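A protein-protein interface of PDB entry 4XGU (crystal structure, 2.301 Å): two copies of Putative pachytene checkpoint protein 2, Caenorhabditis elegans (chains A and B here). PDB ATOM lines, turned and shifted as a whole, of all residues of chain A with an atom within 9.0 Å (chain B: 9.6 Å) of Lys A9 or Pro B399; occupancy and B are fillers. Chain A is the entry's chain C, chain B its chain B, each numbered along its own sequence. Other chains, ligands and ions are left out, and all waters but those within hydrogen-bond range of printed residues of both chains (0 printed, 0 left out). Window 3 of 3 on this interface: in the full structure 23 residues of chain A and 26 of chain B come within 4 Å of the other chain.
The backbone carbonyl oxygen (O) of Pro B399 sits close to the side-chain amide nitrogen (ND2) of Asn A10 (3.4 Å).
The side-chain hydroxyl (OH) of Tyr B395 is in hydrogen-bond range of the guanidinium group (NE) of Arg A158 (3.5 Å).
The side-chain hydroxyl of Ser B398 lies within hydrogen-bond range of the backbone carbonyl oxygen of Tyr B395 (3.0 Å).
The side-chain amide oxygen (OD1) of Asn A10 is in hydrogen-bond range of a ring nitrogen (NE2) of His A12, 3.1 Å away.
The backbone carbonyl oxygen (O) of Asn A10 is in hydrogen-bond range of the side-chain hydroxyl (OG1) of Thr A73, 2.7 Å away.
O of Leu B393 is in hydrogen-bond range of OG of Ser B396 (2.7 Å).
N of Lys A9 lies within hydrogen-bond range of OE2 of Glu A75 (3.3 Å).
OG of Ser A151 is in hydrogen-bond range of SG of Cys A74, at 3.1 Å.
Lys A9 touches Pro B399 (CB to CB, 3.97 Å).
CB of Ser B396 touches O of Ser A151, at 3.5 Å.
Lys A9 touches one residue of chain B.
Thr A73 touches none of the printed residues of chain B.
Of the printed residues of chain B, Arg A158 touches Tyr B395 (3.3 Å).
Of the printed residues of chain A, Tyr B395 touches Arg A158 (3.3 Å).
Printed residues of chain A within 4 Å of Ser B396: Ser A151 (3.5 Å).
No residue of chain A comes within 4 Å of Ser B398.
Pro B399 touches just these residues of chain A: Lys A9 (3.97 Å) and Asn A10 (3.1 Å).
Glu B400 touches none of the printed residues of chain A.
The nearest residue of chain B that does not touch Lys A9 is Glu B400 (4.6 Å).
The nearest residue of chain A that does not touch Pro B399 is Glu A75 (4.6 Å).
Printed residues of chain B that touch a printed residue of chain A: Tyr B395, Ser B396 and Pro B399.
Of the 16 printed residues of chain A, 4 touch a printed residue of chain B.
Among the printed residues, 4 pairs touch across the chains.
Among the printed residues, no Asp or Glu carboxylate lies within 4 Å of a Lys or Arg side-chain nitrogen of the other chain.
No position is printed for both chains.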
ATOM      1  N   LYS A   9      16.176 -26.948   2.795  1.00  0.00           N
ATOM      2  CA  LYS A   9      17.346 -26.091   2.630  1.00  0.00           C
ATOM      3  C   LYS A   9      17.345 -24.950   3.643  1.00  0.00           C
ATOM      4  O   LYS A   9      18.389 -24.584   4.181  1.00  0.00           O
ATOM      5  CB  LYS A   9      17.404 -25.528   1.207  1.00  0.00           C
ATOM      6  N   ASN A  10      16.163 -24.397   3.897  1.00  0.00           N
ATOM      7  CA  ASN A  10      16.014 -23.292   4.838  1.00  0.00           C
ATOM      8  C   ASN A  10      14.773 -23.448   5.708  1.00  0.00           C
ATOM      9  O   ASN A  10      13.667 -23.113   5.287  1.00  0.00           O
ATOM     10  CB  ASN A  10      15.947 -21.963   4.089  1.00  0.00           C
ATOM     11  CG  ASN A  10      15.765 -20.780   5.020  1.00  0.00           C
ATOM     12  OD1 ASN A  10      16.270 -20.774   6.143  1.00  0.00           O
ATOM     13  ND2 ASN A  10      15.031 -19.772   4.559  1.00  0.00           N
ATOM     14  N   ILE A  11      14.957 -23.960   6.920  1.00  0.00           N
ATOM     15  CA  ILE A  11      13.836 -24.199   7.822  1.00  0.00           C
ATOM     16  C   ILE A  11      14.147 -23.747   9.248  1.00  0.00           C
ATOM     17  O   ILE A  11      15.193 -24.089   9.804  1.00  0.00           O
ATOM     18  CB  ILE A  11      13.441 -25.690   7.835  1.00  0.00           C
ATOM     19  CG1 ILE A  11      12.946 -26.116   6.451  1.00  0.00           C
ATOM     20  CG2 ILE A  11      12.375 -25.954   8.883  1.00  0.00           C
ATOM     21  CD1 ILE A  11      12.501 -27.557   6.377  1.00  0.00           C
ATOM     22  N   HIS A  12      13.235 -22.974   9.831  1.00  0.00           N
ATOM     23  CA  HIS A  12      13.389 -22.509  11.206  1.00  0.00           C
ATOM     24  C   HIS A  12      12.356 -23.154  12.119  1.00  0.00           C
ATOM     25  O   HIS A  12      11.377 -23.740  11.656  1.00  0.00           O
ATOM     26  CB  HIS A  12      13.270 -20.987  11.278  1.00  0.00           C
ATOM     27  CG  HIS A  12      14.272 -20.264  10.435  1.00  0.00           C
ATOM     28  ND1 HIS A  12      15.300 -19.520  10.974  1.00  0.00           N
ATOM     29  CD2 HIS A  12      14.407 -20.174   9.092  1.00  0.00           C
ATOM     30  CE1 HIS A  12      16.021 -19.000   9.997  1.00  0.00           C
ATOM     31  NE2 HIS A  12      15.503 -19.383   8.845  1.00  0.00           N
ATOM     32  N   GLY A  72       8.510 -23.263  10.198  1.00  0.00           N
ATOM     33  CA  GLY A  72       8.232 -22.438   9.039  1.00  0.00           C
ATOM     34  C   GLY A  72       9.359 -22.382   8.026  1.00  0.00           C
ATOM     35  O   GLY A  72      10.536 -22.302   8.384  1.00  0.00           O
ATOM     36  N   THR A  73       8.990 -22.424   6.752  1.00  0.00           N
ATOM     37  CA  THR A  73       9.954 -22.295   5.669  1.00  0.00           C
ATOM     38  C   THR A  73       9.362 -21.481   4.519  1.00  0.00           C
ATOM     39  O   THR A  73       8.194 -21.642   4.163  1.00  0.00           O
ATOM     40  CB  THR A  73      10.416 -23.671   5.153  1.00  0.00           C
ATOM     41  OG1 THR A  73      11.273 -23.492   4.018  1.00  0.00           O
ATOM     42  CG2 THR A  73       9.222 -24.535   4.761  1.00  0.00           C
ATOM     43  N   CYS A  74      10.177 -20.604   3.944  1.00  0.00           N
ATOM     44  CA  CYS A  74       9.710 -19.689   2.910  1.00  0.00           C
ATOM     45  C   CYS A  74       9.719 -20.314   1.518  1.00  0.00           C
ATOM     46  O   CYS A  74       9.105 -19.780   0.591  1.00  0.00           O
ATOM     47  CB  CYS A  74      10.560 -18.417   2.910  1.00  0.00           C
ATOM     48  SG  CYS A  74      10.302 -17.352   4.350  1.00  0.00           S
ATOM     49  N   GLU A  75      10.413 -21.438   1.369  1.00  0.00           N
ATOM     50  CA  GLU A  75      10.494 -22.101   0.073  1.00  0.00           C
ATOM     51  C   GLU A  75       9.213 -22.884  -0.219  1.00  0.00           C
ATOM     52  O   GLU A  75       8.852 -23.081  -1.379  1.00  0.00           O
ATOM     53  CB  GLU A  75      11.715 -23.025   0.011  1.00  0.00           C
ATOM     54  CG  GLU A  75      11.668 -24.188   0.987  1.00  0.00           C
ATOM     55  CD  GLU A  75      12.937 -25.024   0.983  1.00  0.00           C
ATOM     56  OE1 GLU A  75      13.721 -24.926   0.014  1.00  0.00           O
ATOM     57  OE2 GLU A  75      13.151 -25.781   1.956  1.00  0.00           O
ATOM     58  N   LEU A  76       8.528 -23.323   0.834  1.00  0.00           N
ATOM     59  CA  LEU A  76       7.254 -24.021   0.680  1.00  0.00           C
ATOM     60  C   LEU A  76       6.072 -23.064   0.768  1.00  0.00           C
ATOM     61  O   LEU A  76       6.174 -21.996   1.367  1.00  0.00           O
ATOM     62  CB  LEU A  76       7.097 -25.114   1.736  1.00  0.00           C
ATOM     63  CG  LEU A  76       7.792 -26.450   1.477  1.00  0.00           C
ATOM     64  CD1 LEU A  76       7.155 -27.532   2.333  1.00  0.00           C
ATOM     65  CD2 LEU A  76       7.727 -26.814   0.002  1.00  0.00           C
ATOM     66  N   THR A  89      18.330 -31.344   8.577  1.00  0.00           N
ATOM     67  CA  THR A  89      17.731 -30.074   8.178  1.00  0.00           C
ATOM     68  C   THR A  89      17.398 -29.200   9.385  1.00  0.00           C
ATOM     69  O   THR A  89      16.305 -28.642   9.475  1.00  0.00           O
ATOM     70  CB  THR A  89      16.451 -30.292   7.348  1.00  0.00           C
ATOM     71  OG1 THR A  89      15.812 -31.508   7.760  1.00  0.00           O
ATOM     72  CG2 THR A  89      16.789 -30.385   5.867  1.00  0.00           C
ATOM     73  N   ILE A  90      18.353 -29.076  10.303  1.00  0.00           N
ATOM     74  CA  ILE A  90      18.156 -28.319  11.535  1.00  0.00           C
ATOM     75  C   ILE A  90      19.457 -27.681  12.021  1.00  0.00           C
ATOM     76  O   ILE A  90      20.501 -28.331  12.062  1.00  0.00           O
ATOM     77  CB  ILE A  90      17.582 -29.218  12.655  1.00  0.00           C
ATOM     78  CG1 ILE A  90      16.066 -29.357  12.512  1.00  0.00           C
ATOM     79  CG2 ILE A  90      17.919 -28.663  14.030  1.00  0.00           C
ATOM     80  CD1 ILE A  90      15.442 -30.285  13.533  1.00  0.00           C
ATOM     81  N   ASN A  91      19.389 -26.402  12.377  1.00  0.00           N
ATOM     82  CA  ASN A  91      20.519 -25.724  13.002  1.00  0.00           C
ATOM     83  C   ASN A  91      20.148 -25.210  14.386  1.00  0.00           C
ATOM     84  O   ASN A  91      19.049 -24.694  14.580  1.00  0.00           O
ATOM     85  CB  ASN A  91      21.009 -24.569  12.127  1.00  0.00           C
ATOM     86  CG  ASN A  91      21.719 -25.047  10.878  1.00  0.00           C
ATOM     87  OD1 ASN A  91      22.944 -24.961  10.774  1.00  0.00           O
ATOM     88  ND2 ASN A  91      20.954 -25.562   9.923  1.00  0.00           N
ATOM     89  N   ASN A  94      19.184 -21.877  13.924  1.00  0.00           N
ATOM     90  CA  ASN A  94      17.914 -21.816  13.208  1.00  0.00           C
ATOM     91  C   ASN A  94      16.731 -22.184  14.097  1.00  0.00           C
ATOM     92  O   ASN A  94      15.591 -21.831  13.807  1.00  0.00           O
ATOM     93  CB  ASN A  94      17.934 -22.738  11.987  1.00  0.00           C
ATOM     94  CG  ASN A  94      18.359 -22.025  10.724  1.00  0.00           C
ATOM     95  OD1 ASN A  94      18.360 -20.796  10.661  1.00  0.00           O
ATOM     96  ND2 ASN A  94      18.711 -22.795   9.700  1.00  0.00           N
ATOM     97  N   SER A 151      10.233 -13.112   3.868  1.00  0.00           N
ATOM     98  CA  SER A 151      11.575 -13.300   3.319  1.00  0.00           C
ATOM     99  C   SER A 151      12.312 -11.985   3.127  1.00  0.00           C
ATOM    100  O   SER A 151      13.493 -11.869   3.458  1.00  0.00           O
ATOM    101  CB  SER A 151      11.513 -14.038   1.980  1.00  0.00           C
ATOM    102  OG  SER A 151      10.987 -15.341   2.136  1.00  0.00           O
ATOM    103  N   ARG A 158      18.604  -9.125   8.567  1.00  0.00           N
ATOM    104  CA  ARG A 158      19.919  -9.761   8.596  1.00  0.00           C
ATOM    105  C   ARG A 158      21.009  -8.818   8.086  1.00  0.00           C
ATOM    106  O   ARG A 158      22.058  -8.680   8.718  1.00  0.00           O
ATOM    107  CB  ARG A 158      19.906 -11.055   7.776  1.00  0.00           C
ATOM    108  CG  ARG A 158      19.256 -12.234   8.491  1.00  0.00           C
ATOM    109  CD  ARG A 158      18.212 -12.924   7.620  1.00  0.00           C
ATOM    110  NE  ARG A 158      18.797 -13.726   6.547  1.00  0.00           N
ATOM    111  CZ  ARG A 158      18.112 -14.191   5.506  1.00  0.00           C
ATOM    112  NH1 ARG A 158      16.817 -13.923   5.387  1.00  0.00           N
ATOM    113  NH2 ARG A 158      18.720 -14.917   4.577  1.00  0.00           N
ATOM    114  N   ARG A 199      13.049 -14.925  15.465  1.00  0.00           N
ATOM    115  CA  ARG A 199      14.092 -15.343  14.533  1.00  0.00           C
ATOM    116  C   ARG A 199      15.434 -14.673  14.849  1.00  0.00           C
ATOM    117  O   ARG A 199      16.494 -15.275  14.668  1.00  0.00           O
ATOM    118  CB  ARG A 199      13.674 -15.033  13.091  1.00  0.00           C
ATOM    119  CG  ARG A 199      14.701 -15.431  12.037  1.00  0.00           C
ATOM    120  CD  ARG A 199      14.384 -14.805  10.682  1.00  0.00           C
ATOM    121  NE  ARG A 199      13.236 -15.431  10.030  1.00  0.00           N
ATOM    122  CZ  ARG A 199      13.279 -15.994   8.827  1.00  0.00           C
ATOM    123  NH1 ARG A 199      14.414 -16.004   8.137  1.00  0.00           N
ATOM    124  NH2 ARG A 199      12.187 -16.540   8.310  1.00  0.00           N
ATOM    125  N   LEU B 393      17.104  -7.858  -2.399  1.00  0.00           N
ATOM    126  CA  LEU B 393      16.148  -8.714  -3.090  1.00  0.00           C
ATOM    127  C   LEU B 393      16.773 -10.079  -3.349  1.00  0.00           C
ATOM    128  O   LEU B 393      16.102 -11.108  -3.265  1.00  0.00           O
ATOM    129  CB  LEU B 393      15.692  -8.077  -4.406  1.00  0.00           C
ATOM    130  CG  LEU B 393      14.700  -8.882  -5.251  1.00  0.00           C
ATOM    131  CD1 LEU B 393      13.433  -9.194  -4.465  1.00  0.00           C
ATOM    132  CD2 LEU B 393      14.363  -8.140  -6.535  1.00  0.00           C
ATOM    133  N   VAL B 394      18.064 -10.078  -3.661  1.00  0.00           N
ATOM    134  CA  VAL B 394      18.802 -11.313  -3.894  1.00  0.00           C
ATOM    135  C   VAL B 394      18.892 -12.140  -2.614  1.00  0.00           C
ATOM    136  O   VAL B 394      18.784 -13.367  -2.642  1.00  0.00           O
ATOM    137  CB  VAL B 394      20.222 -11.024  -4.424  1.00  0.00           C
ATOM    138  CG1 VAL B 394      21.012 -12.313  -4.580  1.00  0.00           C
ATOM    139  CG2 VAL B 394      20.150 -10.277  -5.747  1.00  0.00           C
ATOM    140  N   TYR B 395      19.075 -11.454  -1.491  1.00  0.00           N
ATOM    141  CA  TYR B 395      19.208 -12.108  -0.195  1.00  0.00           C
ATOM    142  C   TYR B 395      17.939 -12.856   0.202  1.00  0.00           C
ATOM    143  O   TYR B 395      18.002 -13.935   0.793  1.00  0.00           O
ATOM    144  CB  TYR B 395      19.554 -11.076   0.879  1.00  0.00           C
ATOM    145  CG  TYR B 395      20.223 -11.660   2.101  1.00  0.00           C
ATOM    146  CD1 TYR B 395      20.721 -12.955   2.090  1.00  0.00           C
ATOM    147  CD2 TYR B 395      20.353 -10.915   3.266  1.00  0.00           C
ATOM    148  CE1 TYR B 395      21.334 -13.492   3.203  1.00  0.00           C
ATOM    149  CE2 TYR B 395      20.964 -11.443   4.386  1.00  0.00           C
ATOM    150  CZ  TYR B 395      21.453 -12.732   4.348  1.00  0.00           C
ATOM    151  OH  TYR B 395      22.063 -13.265   5.462  1.00  0.00           O
ATOM    152  N   SER B 396      16.787 -12.277  -0.122  1.00  0.00           N
ATOM    153  CA  SER B 396      15.504 -12.870   0.240  1.00  0.00           C
ATOM    154  C   SER B 396      15.207 -14.126  -0.577  1.00  0.00           C
ATOM    155  O   SER B 396      14.578 -15.063  -0.082  1.00  0.00           O
ATOM    156  CB  SER B 396      14.377 -11.853   0.060  1.00  0.00           C
ATOM    157  OG  SER B 396      14.233 -11.493  -1.303  1.00  0.00           O
ATOM    158  N   LYS B 397      15.660 -14.138  -1.826  1.00  0.00           N
ATOM    159  CA  LYS B 397      15.445 -15.279  -2.710  1.00  0.00           C
ATOM    160  C   LYS B 397      16.233 -16.511  -2.271  1.00  0.00           C
ATOM    161  O   LYS B 397      15.753 -17.640  -2.394  1.00  0.00           O
ATOM    162  CB  LYS B 397      15.818 -14.921  -4.150  1.00  0.00           C
ATOM    163  CG  LYS B 397      14.886 -13.928  -4.814  1.00  0.00           C
ATOM    164  CD  LYS B 397      15.060 -13.954  -6.323  1.00  0.00           C
ATOM    165  CE  LYS B 397      13.961 -13.168  -7.020  1.00  0.00           C
ATOM    166  NZ  LYS B 397      13.489 -13.866  -8.249  1.00  0.00           N
ATOM    167  N   SER B 398      17.441 -16.292  -1.763  1.00  0.00           N
ATOM    168  CA  SER B 398      18.314 -17.395  -1.379  1.00  0.00           C
ATOM    169  C   SER B 398      17.757 -18.171  -0.195  1.00  0.00           C
ATOM    170  O   SER B 398      17.500 -17.594   0.863  1.00  0.00           O
ATOM    171  CB  SER B 398      19.712 -16.885  -1.034  1.00  0.00           C
ATOM    172  OG  SER B 398      19.729 -16.305   0.259  1.00  0.00           O
ATOM    173  N   PRO B 399      17.565 -19.487  -0.373  1.00  0.00           N
ATOM    174  CA  PRO B 399      17.182 -20.350   0.746  1.00  0.00           C
ATOM    175  C   PRO B 399      18.265 -20.357   1.819  1.00  0.00           C
ATOM    176  O   PRO B 399      18.010 -19.967   2.958  1.00  0.00           O
ATOM    177  CB  PRO B 399      17.040 -21.733   0.099  1.00  0.00           C
ATOM    178  CG  PRO B 399      16.822 -21.457  -1.354  1.00  0.00           C
ATOM    179  CD  PRO B 399      17.627 -20.227  -1.645  1.00  0.00           C
ATOM    180  N   GLU B 400      19.467 -20.778   1.437  1.00  0.00           N
ATOM    181  CA  GLU B 400      20.594 -20.873   2.359  1.00  0.00           C
ATOM    182  C   GLU B 400      20.881 -19.553   3.072  1.00  0.00           C
ATOM    183  O   GLU B 400      20.603 -18.474   2.545  1.00  0.00           O
ATOM    184  CB  GLU B 400      21.851 -21.338   1.617  1.00  0.00           C
ATOM    185  CG  GLU B 400      21.784 -22.757   1.057  1.00  0.00           C
ATOM    186  CD  GLU B 400      21.031 -22.849  -0.259  1.00  0.00           C
ATOM    187  OE1 GLU B 400      20.363 -21.866  -0.645  1.00  0.00           O
ATOM    188  OE2 GLU B 400      21.113 -23.910  -0.913  1.00  0.00           O
ATOM    189  N   GLU B 401      21.434 -19.655   4.277  1.00  0.00           N
ATOM    190  CA  GLU B 401      21.824 -18.487   5.060  1.00  0.00           C
ATOM    191  C   GLU B 401      22.986 -17.765   4.389  1.00  0.00           C
ATOM    192  O   GLU B 401      23.178 -16.561   4.562  1.00  0.00           O
ATOM    193  CB  GLU B 401      22.211 -18.904   6.480  1.00  0.00           C
ATOM    194  CG  GLU B 401      22.268 -17.764   7.482  1.00  0.00           C
ATOM    195  CD  GLU B 401      20.934 -17.519   8.159  1.00  0.00           C
ATOM    196  OE1 GLU B 401      20.825 -16.534   8.920  1.00  0.00           O
ATOM    197  OE2 GLU B 401      19.995 -18.316   7.936  1.00  0.00           O
ATOM    198  N   THR B 402      23.759 -18.525   3.620  1.00  0.00           N
ATOM    199  CA  THR B 402      24.931 -18.006   2.931  1.00  0.00           C
ATOM    200  C   THR B 402      24.911 -18.412   1.460  1.00  0.00           C
ATOM    201  O   THR B 402      24.638 -19.567   1.132  1.00  0.00           O
ATOM    202  CB  THR B 402      26.225 -18.509   3.586  1.00  0.00           C
ATOM    203  OG1 THR B 402      26.340 -17.953   4.902  1.00  0.00           O
ATOM    204  CG2 THR B 402      27.432 -18.102   2.764  1.00  0.00           C
ATOM    205  N   ILE B 403      25.200 -17.462   0.578  1.00  0.00           N
ATOM    206  CA  ILE B 403      25.144 -17.718  -0.855  1.00  0.00           C
ATOM    207  C   ILE B 403      26.512 -18.057  -1.441  1.00  0.00           C
ATOM    208  O   ILE B 403      27.496 -17.362  -1.188  1.00  0.00           O
ATOM    209  CB  ILE B 403      24.567 -16.508  -1.610  1.00  0.00           C
ATOM    210  CG1 ILE B 403      23.301 -16.004  -0.919  1.00  0.00           C
ATOM    211  CG2 ILE B 403      24.278 -16.870  -3.056  1.00  0.00           C
ATOM    212  CD1 ILE B 403      22.658 -14.829  -1.617  1.00  0.00           C
ATOM    213  N   THR B 404      26.566 -19.130  -2.224  1.00  0.00           N
ATOM    214  CA  THR B 404      27.778 -19.472  -2.960  1.00  0.00           C
ATOM    215  C   THR B 404      27.945 -18.498  -4.121  1.00  0.00           C
ATOM    216  O   THR B 404      26.965 -17.933  -4.607  1.00  0.00           O
ATOM    217  CB  THR B 404      27.737 -20.918  -3.497  1.00  0.00           C
ATOM    218  OG1 THR B 404      26.920 -20.975  -4.673  1.00  0.00           O
ATOM    219  CG2 THR B 404      27.176 -21.864  -2.443  1.00  0.00           C
ATOM    220  N   ASN B 407      26.000 -19.473  -7.378  1.00  0.00           N
ATOM    221  CA  ASN B 407      24.575 -19.229  -7.188  1.00  0.00           C
ATOM    222  C   ASN B 407      24.267 -17.739  -7.091  1.00  0.00           C
ATOM    223  O   ASN B 407      23.217 -17.281  -7.544  1.00  0.00           O
ATOM    224  CB  ASN B 407      24.068 -19.951  -5.939  1.00  0.00           C
ATOM    225  CG  ASN B 407      23.092 -21.061  -6.270  1.00  0.00           C
ATOM    226  OD1 ASN B 407      22.399 -21.009  -7.286  1.00  0.00           O
ATOM    227  ND2 ASN B 407      23.031 -22.073  -5.411  1.00  0.00           N
ATOM    228  N   CYS B 408      25.193 -16.991  -6.499  1.00  0.00           N
ATOM    229  CA  CYS B 408      25.051 -15.547  -6.352  1.00  0.00           C
ATOM    230  C   CYS B 408      24.863 -14.860  -7.698  1.00  0.00           C
ATOM    231  O   CYS B 408      24.027 -13.969  -7.842  1.00  0.00           O
ATOM    232  CB  CYS B 408      26.269 -14.967  -5.638  1.00  0.00           C
ATOM    233  SG  CYS B 408      26.394 -13.177  -5.747  1.00  0.00           S
ATOM    234  N   LEU B 411      21.381 -15.773  -8.910  1.00  0.00           N
ATOM    235  CA  LEU B 411      20.320 -15.073  -8.193  1.00  0.00           C
ATOM    236  C   LEU B 411      20.265 -13.604  -8.588  1.00  0.00           C
ATOM    237  O   LEU B 411      19.184 -13.037  -8.752  1.00  0.00           O
ATOM    238  CB  LEU B 411      20.506 -15.200  -6.680  1.00  0.00           C
ATOM    239  CG  LEU B 411      20.376 -16.601  -6.076  1.00  0.00           C
ATOM    240  CD1 LEU B 411      20.315 -16.524  -4.558  1.00  0.00           C
ATOM    241  CD2 LEU B 411      19.161 -17.333  -6.635  1.00  0.00           C
ATOM    242  N   GLU B 414      18.467 -13.194 -11.791  1.00  0.00           N
ATOM    243  CA  GLU B 414      17.027 -13.349 -11.623  1.00  0.00           C
ATOM    244  C   GLU B 414      16.390 -12.085 -11.059  1.00  0.00           C
ATOM    245  O   GLU B 414      15.311 -11.678 -11.493  1.00  0.00           O
ATOM    246  CB  GLU B 414      16.712 -14.538 -10.718  1.00  0.00           C
ATOM    247  CG  GLU B 414      16.495 -15.841 -11.465  1.00  0.00           C
ATOM    248  CD  GLU B 414      15.400 -16.684 -10.846  1.00  0.00           C
ATOM    249  OE1 GLU B 414      14.829 -17.538 -11.560  1.00  0.00           O
ATOM    250  OE2 GLU B 414      15.106 -16.492  -9.646  1.00  0.00           O
